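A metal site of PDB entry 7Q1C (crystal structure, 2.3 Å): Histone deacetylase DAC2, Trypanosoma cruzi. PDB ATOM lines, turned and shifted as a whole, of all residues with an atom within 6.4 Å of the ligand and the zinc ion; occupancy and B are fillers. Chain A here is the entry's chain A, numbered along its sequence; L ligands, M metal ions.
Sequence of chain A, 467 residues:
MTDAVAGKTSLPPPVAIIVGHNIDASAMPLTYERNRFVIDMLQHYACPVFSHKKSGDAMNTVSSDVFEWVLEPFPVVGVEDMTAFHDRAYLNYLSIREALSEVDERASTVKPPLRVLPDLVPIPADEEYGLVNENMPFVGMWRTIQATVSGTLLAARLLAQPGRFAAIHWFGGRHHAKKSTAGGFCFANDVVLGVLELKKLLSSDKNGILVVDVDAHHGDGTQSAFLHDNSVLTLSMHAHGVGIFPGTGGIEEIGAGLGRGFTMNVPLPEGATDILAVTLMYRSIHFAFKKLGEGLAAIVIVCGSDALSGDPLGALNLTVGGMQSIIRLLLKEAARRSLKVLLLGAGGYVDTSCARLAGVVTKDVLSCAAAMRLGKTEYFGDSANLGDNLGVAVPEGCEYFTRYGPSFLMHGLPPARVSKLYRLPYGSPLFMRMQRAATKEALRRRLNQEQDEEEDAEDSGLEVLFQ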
ATOM      1  N   GLU A 134       1.809  18.203  32.473  1.00  0.00           N
ATOM      2  CA  GLU A 134       1.803  19.478  31.780  1.00  0.00           C
ATOM      3  C   GLU A 134       0.638  19.588  30.817  1.00  0.00           C
ATOM      4  O   GLU A 134       0.248  20.711  30.476  1.00  0.00           O
ATOM      5  CB  GLU A 134       3.141  19.693  31.043  1.00  0.00           C
ATOM      6  CG  GLU A 134       3.388  18.823  29.794  1.00  0.00           C
ATOM      7  CD  GLU A 134       4.045  17.468  30.108  1.00  0.00           C
ATOM      8  OE1 GLU A 134       4.157  17.102  31.309  1.00  0.00           O
ATOM      9  OE2 GLU A 134       4.449  16.757  29.141  1.00  0.00           O
ATOM     10  N   GLY A 173       2.485  26.265  16.146  1.00  0.00           N
ATOM     11  CA  GLY A 173       3.732  25.542  16.328  1.00  0.00           C
ATOM     12  C   GLY A 173       3.762  24.538  17.458  1.00  0.00           C
ATOM     13  O   GLY A 173       4.804  24.346  18.087  1.00  0.00           O
ATOM     14  N   ARG A 174       2.644  23.862  17.705  1.00  0.00           N
ATOM     15  CA  ARG A 174       2.549  22.848  18.763  1.00  0.00           C
ATOM     16  C   ARG A 174       3.135  21.515  18.272  1.00  0.00           C
ATOM     17  O   ARG A 174       2.438  20.532  18.001  1.00  0.00           O
ATOM     18  CB  ARG A 174       1.100  22.689  19.201  1.00  0.00           C
ATOM     19  CG  ARG A 174       0.443  23.961  19.687  1.00  0.00           C
ATOM     20  CD  ARG A 174       1.188  24.539  20.868  1.00  0.00           C
ATOM     21  NE  ARG A 174       1.223  26.004  20.785  1.00  0.00           N
ATOM     22  CZ  ARG A 174       2.328  26.728  20.610  1.00  0.00           C
ATOM     23  NH1 ARG A 174       3.533  26.181  20.542  1.00  0.00           N
ATOM     24  NH2 ARG A 174       2.216  28.053  20.539  1.00  0.00           N
ATOM     25  N   HIS A 175       4.459  21.465  18.201  1.00  0.00           N
ATOM     26  CA  HIS A 175       5.150  20.402  17.477  1.00  0.00           C
ATOM     27  C   HIS A 175       5.266  19.085  18.255  1.00  0.00           C
ATOM     28  O   HIS A 175       5.741  18.099  17.690  1.00  0.00           O
ATOM     29  CB  HIS A 175       6.553  20.891  17.087  1.00  0.00           C
ATOM     30  CG  HIS A 175       7.390  21.280  18.273  1.00  0.00           C
ATOM     31  ND1 HIS A 175       8.751  21.429  18.199  1.00  0.00           N
ATOM     32  CD2 HIS A 175       7.055  21.527  19.559  1.00  0.00           C
ATOM     33  CE1 HIS A 175       9.224  21.755  19.387  1.00  0.00           C
ATOM     34  NE2 HIS A 175       8.210  21.826  20.233  1.00  0.00           N
ATOM     35  N   HIS A 176       4.845  19.044  19.522  1.00  0.00           N
ATOM     36  CA  HIS A 176       4.987  17.818  20.311  1.00  0.00           C
ATOM     37  C   HIS A 176       3.813  16.873  20.217  1.00  0.00           C
ATOM     38  O   HIS A 176       3.925  15.712  20.619  1.00  0.00           O
ATOM     39  CB  HIS A 176       5.183  18.141  21.793  1.00  0.00           C
ATOM     40  CG  HIS A 176       6.520  18.701  22.122  1.00  0.00           C
ATOM     41  ND1 HIS A 176       7.696  18.054  21.793  1.00  0.00           N
ATOM     42  CD2 HIS A 176       6.878  19.820  22.776  1.00  0.00           C
ATOM     43  CE1 HIS A 176       8.723  18.772  22.228  1.00  0.00           C
ATOM     44  NE2 HIS A 176       8.246  19.839  22.828  1.00  0.00           N
ATOM     45  N   GLY A 183       1.320  16.198  24.469  1.00  0.00           N
ATOM     46  CA  GLY A 183       2.636  16.252  25.079  1.00  0.00           C
ATOM     47  C   GLY A 183       3.244  17.641  25.046  1.00  0.00           C
ATOM     48  O   GLY A 183       3.011  18.418  24.105  1.00  0.00           O
ATOM     49  N   GLY A 184       4.034  17.966  26.076  1.00  0.00           N
ATOM     50  CA  GLY A 184       4.699  19.253  26.146  1.00  0.00           C
ATOM     51  C   GLY A 184       3.824  20.432  25.798  1.00  0.00           C
ATOM     52  O   GLY A 184       4.216  21.283  25.004  1.00  0.00           O
ATOM     53  N   PHE A 185       2.616  20.477  26.378  1.00  0.00           N
ATOM     54  CA  PHE A 185       1.617  21.525  26.179  1.00  0.00           C
ATOM     55  C   PHE A 185       0.985  21.507  24.789  1.00  0.00           C
ATOM     56  O   PHE A 185       0.299  22.461  24.433  1.00  0.00           O
ATOM     57  CB  PHE A 185       2.155  22.942  26.427  1.00  0.00           C
ATOM     58  CG  PHE A 185       2.807  23.131  27.762  1.00  0.00           C
ATOM     59  CD1 PHE A 185       2.056  23.089  28.931  1.00  0.00           C
ATOM     60  CD2 PHE A 185       4.165  23.403  27.844  1.00  0.00           C
ATOM     61  CE1 PHE A 185       2.667  23.284  30.175  1.00  0.00           C
ATOM     62  CE2 PHE A 185       4.789  23.598  29.081  1.00  0.00           C
ATOM     63  CZ  PHE A 185       4.043  23.535  30.244  1.00  0.00           C
ATOM     64  N   CYS A 186       1.184  20.471  23.999  1.00  0.00           N
ATOM     65  CA  CYS A 186       0.615  20.439  22.653  1.00  0.00           C
ATOM     66  C   CYS A 186      -0.434  19.338  22.585  1.00  0.00           C
ATOM     67  O   CYS A 186      -0.182  18.195  22.996  1.00  0.00           O
ATOM     68  CB  CYS A 186       1.724  20.221  21.610  1.00  0.00           C
ATOM     69  SG  CYS A 186       3.194  21.337  21.811  1.00  0.00           S
ATOM     70  N   ASP A 215      13.150  25.244  17.971  1.00  0.00           N
ATOM     71  CA  ASP A 215      12.760  25.220  19.373  1.00  0.00           C
ATOM     72  C   ASP A 215      13.809  24.415  20.161  1.00  0.00           C
ATOM     73  O   ASP A 215      14.467  23.536  19.618  1.00  0.00           O
ATOM     74  CB  ASP A 215      11.351  24.608  19.452  1.00  0.00           C
ATOM     75  CG  ASP A 215      10.860  24.442  20.864  1.00  0.00           C
ATOM     76  OD1 ASP A 215      11.300  23.466  21.542  1.00  0.00           O
ATOM     77  OD2 ASP A 215      10.007  25.277  21.289  1.00  0.00           O
ATOM     78  N   ALA A 216      13.971  24.734  21.457  1.00  0.00           N
ATOM     79  CA  ALA A 216      14.962  24.019  22.278  1.00  0.00           C
ATOM     80  C   ALA A 216      14.643  22.544  22.488  1.00  0.00           C
ATOM     81  O   ALA A 216      15.494  21.819  23.027  1.00  0.00           O
ATOM     82  CB  ALA A 216      15.117  24.680  23.636  1.00  0.00           C
ATOM     83  N   HIS A 217      13.452  22.063  22.127  1.00  0.00           N
ATOM     84  CA  HIS A 217      13.047  20.701  22.410  1.00  0.00           C
ATOM     85  C   HIS A 217      12.808  19.933  21.126  1.00  0.00           C
ATOM     86  O   HIS A 217      12.401  20.510  20.112  1.00  0.00           O
ATOM     87  CB  HIS A 217      11.791  20.666  23.289  1.00  0.00           C
ATOM     88  CG  HIS A 217      11.977  21.354  24.601  1.00  0.00           C
ATOM     89  ND1 HIS A 217      11.507  22.630  24.850  1.00  0.00           N
ATOM     90  CD2 HIS A 217      12.603  20.964  25.730  1.00  0.00           C
ATOM     91  CE1 HIS A 217      11.818  22.976  26.081  1.00  0.00           C
ATOM     92  NE2 HIS A 217      12.488  21.990  26.634  1.00  0.00           N
ATOM     93  N   GLY A 243      17.366  13.765  31.508  1.00  0.00           N
ATOM     94  CA  GLY A 243      16.367  14.668  32.042  1.00  0.00           C
ATOM     95  C   GLY A 243      16.130  15.933  31.242  1.00  0.00           C
ATOM     96  O   GLY A 243      15.694  16.944  31.823  1.00  0.00           O
ATOM     97  N   ILE A 244      16.413  15.932  29.939  1.00  0.00           N
ATOM     98  CA  ILE A 244      15.982  17.008  29.043  1.00  0.00           C
ATOM     99  C   ILE A 244      14.770  16.504  28.257  1.00  0.00           C
ATOM    100  O   ILE A 244      14.843  15.469  27.591  1.00  0.00           O
ATOM    101  CB  ILE A 244      17.117  17.474  28.107  1.00  0.00           C
ATOM    102  CG1 ILE A 244      18.104  18.359  28.862  1.00  0.00           C
ATOM    103  CG2 ILE A 244      16.599  18.308  26.949  1.00  0.00           C
ATOM    104  CD1 ILE A 244      19.158  17.612  29.588  1.00  0.00           C
ATOM    105  N   PHE A 245      13.663  17.231  28.344  1.00  0.00           N
ATOM    106  CA  PHE A 245      12.438  16.865  27.652  1.00  0.00           C
ATOM    107  C   PHE A 245      12.635  16.924  26.129  1.00  0.00           C
ATOM    108  O   PHE A 245      13.369  17.772  25.621  1.00  0.00           O
ATOM    109  CB  PHE A 245      11.309  17.806  28.078  1.00  0.00           C
ATOM    110  CG  PHE A 245       9.997  17.538  27.413  1.00  0.00           C
ATOM    111  CD1 PHE A 245       9.111  16.626  27.947  1.00  0.00           C
ATOM    112  CD2 PHE A 245       9.635  18.210  26.263  1.00  0.00           C
ATOM    113  CE1 PHE A 245       7.909  16.363  27.339  1.00  0.00           C
ATOM    114  CE2 PHE A 245       8.423  17.963  25.639  1.00  0.00           C
ATOM    115  CZ  PHE A 245       7.559  17.035  26.182  1.00  0.00           C
ATOM    116  N   GLY A 304      10.883  28.496  17.996  1.00  0.00           N
ATOM    117  CA  GLY A 304      10.701  28.744  19.406  1.00  0.00           C
ATOM    118  C   GLY A 304      11.757  29.694  19.917  1.00  0.00           C
ATOM    119  O   GLY A 304      12.847  29.814  19.355  1.00  0.00           O
ATOM    120  N   ASP A 306      12.625  29.405  23.238  1.00  0.00           N
ATOM    121  CA  ASP A 306      13.156  28.827  24.459  1.00  0.00           C
ATOM    122  C   ASP A 306      14.547  28.246  24.288  1.00  0.00           C
ATOM    123  O   ASP A 306      15.124  27.789  25.286  1.00  0.00           O
ATOM    124  CB  ASP A 306      12.226  27.742  25.015  1.00  0.00           C
ATOM    125  CG  ASP A 306      11.875  26.669  24.010  1.00  0.00           C
ATOM    126  OD1 ASP A 306      12.306  26.718  22.841  1.00  0.00           O
ATOM    127  OD2 ASP A 306      11.115  25.774  24.389  1.00  0.00           O
ATOM    128  N   PRO A 312      13.979  29.530  31.176  1.00  0.00           N
ATOM    129  CA  PRO A 312      13.910  28.643  32.353  1.00  0.00           C
ATOM    130  C   PRO A 312      13.721  27.174  32.004  1.00  0.00           C
ATOM    131  O   PRO A 312      14.096  26.311  32.811  1.00  0.00           O
ATOM    132  CB  PRO A 312      12.723  29.194  33.153  1.00  0.00           C
ATOM    133  CG  PRO A 312      11.914  29.984  32.166  1.00  0.00           C
ATOM    134  CD  PRO A 312      12.907  30.545  31.183  1.00  0.00           C
ATOM    135  N   LEU A 313      13.182  26.841  30.827  1.00  0.00           N
ATOM    136  CA  LEU A 313      12.914  25.456  30.441  1.00  0.00           C
ATOM    137  C   LEU A 313      13.837  24.949  29.353  1.00  0.00           C
ATOM    138  O   LEU A 313      14.320  23.817  29.414  1.00  0.00           O
ATOM    139  CB  LEU A 313      11.460  25.323  29.973  1.00  0.00           C
ATOM    140  CG  LEU A 313      10.440  25.604  31.068  1.00  0.00           C
ATOM    141  CD1 LEU A 313       9.062  25.317  30.504  1.00  0.00           C
ATOM    142  CD2 LEU A 313      10.723  24.714  32.263  1.00  0.00           C
ATOM    143  N   GLY A 314      14.039  25.745  28.298  1.00  0.00           N
ATOM    144  CA  GLY A 314      15.062  25.397  27.340  1.00  0.00           C
ATOM    145  C   GLY A 314      16.398  25.367  28.041  1.00  0.00           C
ATOM    146  O   GLY A 314      16.647  26.124  28.976  1.00  0.00           O
ATOM    147  N   ALA A 346       6.576  28.587  18.721  1.00  0.00           N
ATOM    148  CA  ALA A 346       6.625  27.344  19.499  1.00  0.00           C
ATOM    149  C   ALA A 346       6.742  27.631  20.996  1.00  0.00           C
ATOM    150  O   ALA A 346       5.977  28.441  21.541  1.00  0.00           O
ATOM    151  CB  ALA A 346       7.790  26.456  19.039  1.00  0.00           C
ATOM    152  N   GLY A 347       7.658  26.936  21.677  1.00  0.00           N
ATOM    153  CA  GLY A 347       7.941  27.233  23.064  1.00  0.00           C
ATOM    154  C   GLY A 347       8.666  28.557  23.234  1.00  0.00           C
ATOM    155  O   GLY A 347       9.049  29.223  22.269  1.00  0.00           O
ATOM    156  N   GLY A 348       8.842  28.960  24.487  1.00  0.00           N
ATOM    157  CA  GLY A 348       9.440  30.225  24.853  1.00  0.00           C
ATOM    158  C   GLY A 348       8.818  30.736  26.134  1.00  0.00           C
ATOM    159  O   GLY A 348       7.626  31.030  26.171  1.00  0.00           O
ATOM    160  N   TYR A 349       9.594  30.841  27.210  1.00  0.00           N
ATOM    161  CA  TYR A 349       9.038  31.074  28.531  1.00  0.00           C
ATOM    162  C   TYR A 349       9.612  32.340  29.171  1.00  0.00           C
ATOM    163  O   TYR A 349       9.516  32.518  30.389  1.00  0.00           O
ATOM    164  CB  TYR A 349       9.238  29.822  29.399  1.00  0.00           C
ATOM    165  CG  TYR A 349       8.574  28.677  28.675  1.00  0.00           C
ATOM    166  CD1 TYR A 349       7.185  28.549  28.698  1.00  0.00           C
ATOM    167  CD2 TYR A 349       9.301  27.802  27.867  1.00  0.00           C
ATOM    168  CE1 TYR A 349       6.557  27.566  27.979  1.00  0.00           C
ATOM    169  CE2 TYR A 349       8.678  26.813  27.144  1.00  0.00           C
ATOM    170  CZ  TYR A 349       7.308  26.694  27.204  1.00  0.00           C
ATOM    171  OH  TYR A 349       6.673  25.718  26.489  1.00  0.00           O
ATOM    172  N   ARG A 417      20.831  30.534  32.531  1.00  0.00           N
ATOM    173  CA  ARG A 417      20.399  29.590  33.561  1.00  0.00           C
ATOM    174  C   ARG A 417      21.322  28.385  33.663  1.00  0.00           C
ATOM    175  O   ARG A 417      21.522  27.853  34.759  1.00  0.00           O
ATOM    176  CB  ARG A 417      18.972  29.106  33.314  1.00  0.00           C
ATOM    177  CG  ARG A 417      18.491  28.064  34.333  1.00  0.00           C
ATOM    178  CD  ARG A 417      17.040  27.593  34.101  1.00  0.00           C
ATOM    179  NE  ARG A 417      16.854  26.893  32.833  1.00  0.00           N
ATOM    180  CZ  ARG A 417      17.124  25.606  32.643  1.00  0.00           C
ATOM    181  NH1 ARG A 417      17.642  24.856  33.596  1.00  0.00           N
ATOM    182  NH2 ARG A 417      16.876  25.068  31.454  1.00  0.00           N
HETATM  183  C1  LIG L   1       7.992  22.946  25.244  1.00  0.00           C
HETATM  184  C2  LIG L   1       7.657  22.069  26.450  1.00  0.00           C
HETATM  185  C3  LIG L   1       8.344  22.157  27.569  1.00  0.00           C
HETATM  186  C4  LIG L   1       8.049  21.258  28.773  1.00  0.00           C
HETATM  187  C5  LIG L   1       6.761  20.808  29.005  1.00  0.00           C
HETATM  188  C6  LIG L   1       6.513  19.981  30.092  1.00  0.00           C
HETATM  189  C7  LIG L   1       7.524  19.603  30.950  1.00  0.00           C
HETATM  190  C8  LIG L   1       8.845  20.056  30.735  1.00  0.00           C
HETATM  191  C9  LIG L   1      10.105  19.844  31.428  1.00  0.00           C
HETATM  192  C10 LIG L   1      10.464  19.107  32.582  1.00  0.00           C
HETATM  193  C11 LIG L   1      11.788  19.098  33.018  1.00  0.00           C
HETATM  194  C12 LIG L   1      12.763  19.809  32.317  1.00  0.00           C
HETATM  195  C13 LIG L   1      12.418  20.527  31.188  1.00  0.00           C
HETATM  196  C14 LIG L   1      11.066  20.545  30.744  1.00  0.00           C
HETATM  197  C15 LIG L   1       9.097  20.869  29.656  1.00  0.00           C
HETATM  198  N1  LIG L   1       8.157  22.321  23.937  1.00  0.00           N
HETATM  199  O1  LIG L   1       8.153  24.113  25.348  1.00  0.00           O
HETATM  200  O2  LIG L   1      10.459  21.170  29.672  1.00  0.00           O
HETATM  201  O3  LIG L   1       8.478  23.005  22.735  1.00  0.00           O
HETATM  202 ZN    ZN M   1      10.234  23.932  23.464  1.00  0.00          ZN
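O3 of the ligand sits close to NE2 of His 175, at 2.8 Å. A nitrogen (N1) of the ligand sits at hydrogen-bond distance from a ring nitrogen (NE2) of His 176 (2.7 Å). OH of Tyr 349 lies within hydrogen-bond range of O1 of the ligand (2.5 Å).
N of His 176 sits at hydrogen-bond distance from SG of Cys 186 (3.6 Å). The side-chain carboxylate (OD1) of Asp 306 sits at hydrogen-bond distance from the backbone NH (N) of Ala 216 (2.9 Å). OD2 of Asp 215 sits close to N of Gly 347, at 2.9 Å. The backbone carbonyl oxygen (O) of Gly 184 lies within hydrogen-bond range of the side-chain sulfur (SG) of Cys 186. NE2 of His 176 lies within hydrogen-bond range of NE2 of His 175, 3.3 Å away. OE2 of Glu 134 lies within hydrogen-bond range of N of Gly 184, at 3.3 Å.
Merely in contact with the ligand: Glu 134 (3.3 Å), Phe 185 (3.4 Å), Gly 184 (3.8 Å), Phe 245 (3.8 Å) and Gly 347 (3.9 Å). Hydrophobic or aromatic side chains within 4 Å of the ligand: His 175, His 176, Phe 185, His 217, Phe 245 and Tyr 349. Within 4 Å of the ligand: Glu 134, His 175, His 176, Gly 184, Phe 185, Asp 215, His 217, Phe 245, Asp 306, Gly 347 and Tyr 349.
Three residues have an atom within 4 Å of the zinc ion: Asp 215, His 217 and Asp 306. Along chain A the residues within 4 Å of the zinc ion span positions 215 to 306.
O3 of the ligand binds the zinc ion. OD2 of Asp 306 is bound to the zinc ion (2.2 Å). OD1 of Asp 215 binds the zinc ion (2.2 Å). ND1 of His 217 binds the zinc ion (2.3 Å). The side-chain carboxylate (OD2) of Asp 215 is bound to the zinc ion (2.6 Å). The zinc ion has five donor atoms within binding distance. Slightly farther from the zinc ion lies an oxygen (O1) of the ligand (2.8 Å).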
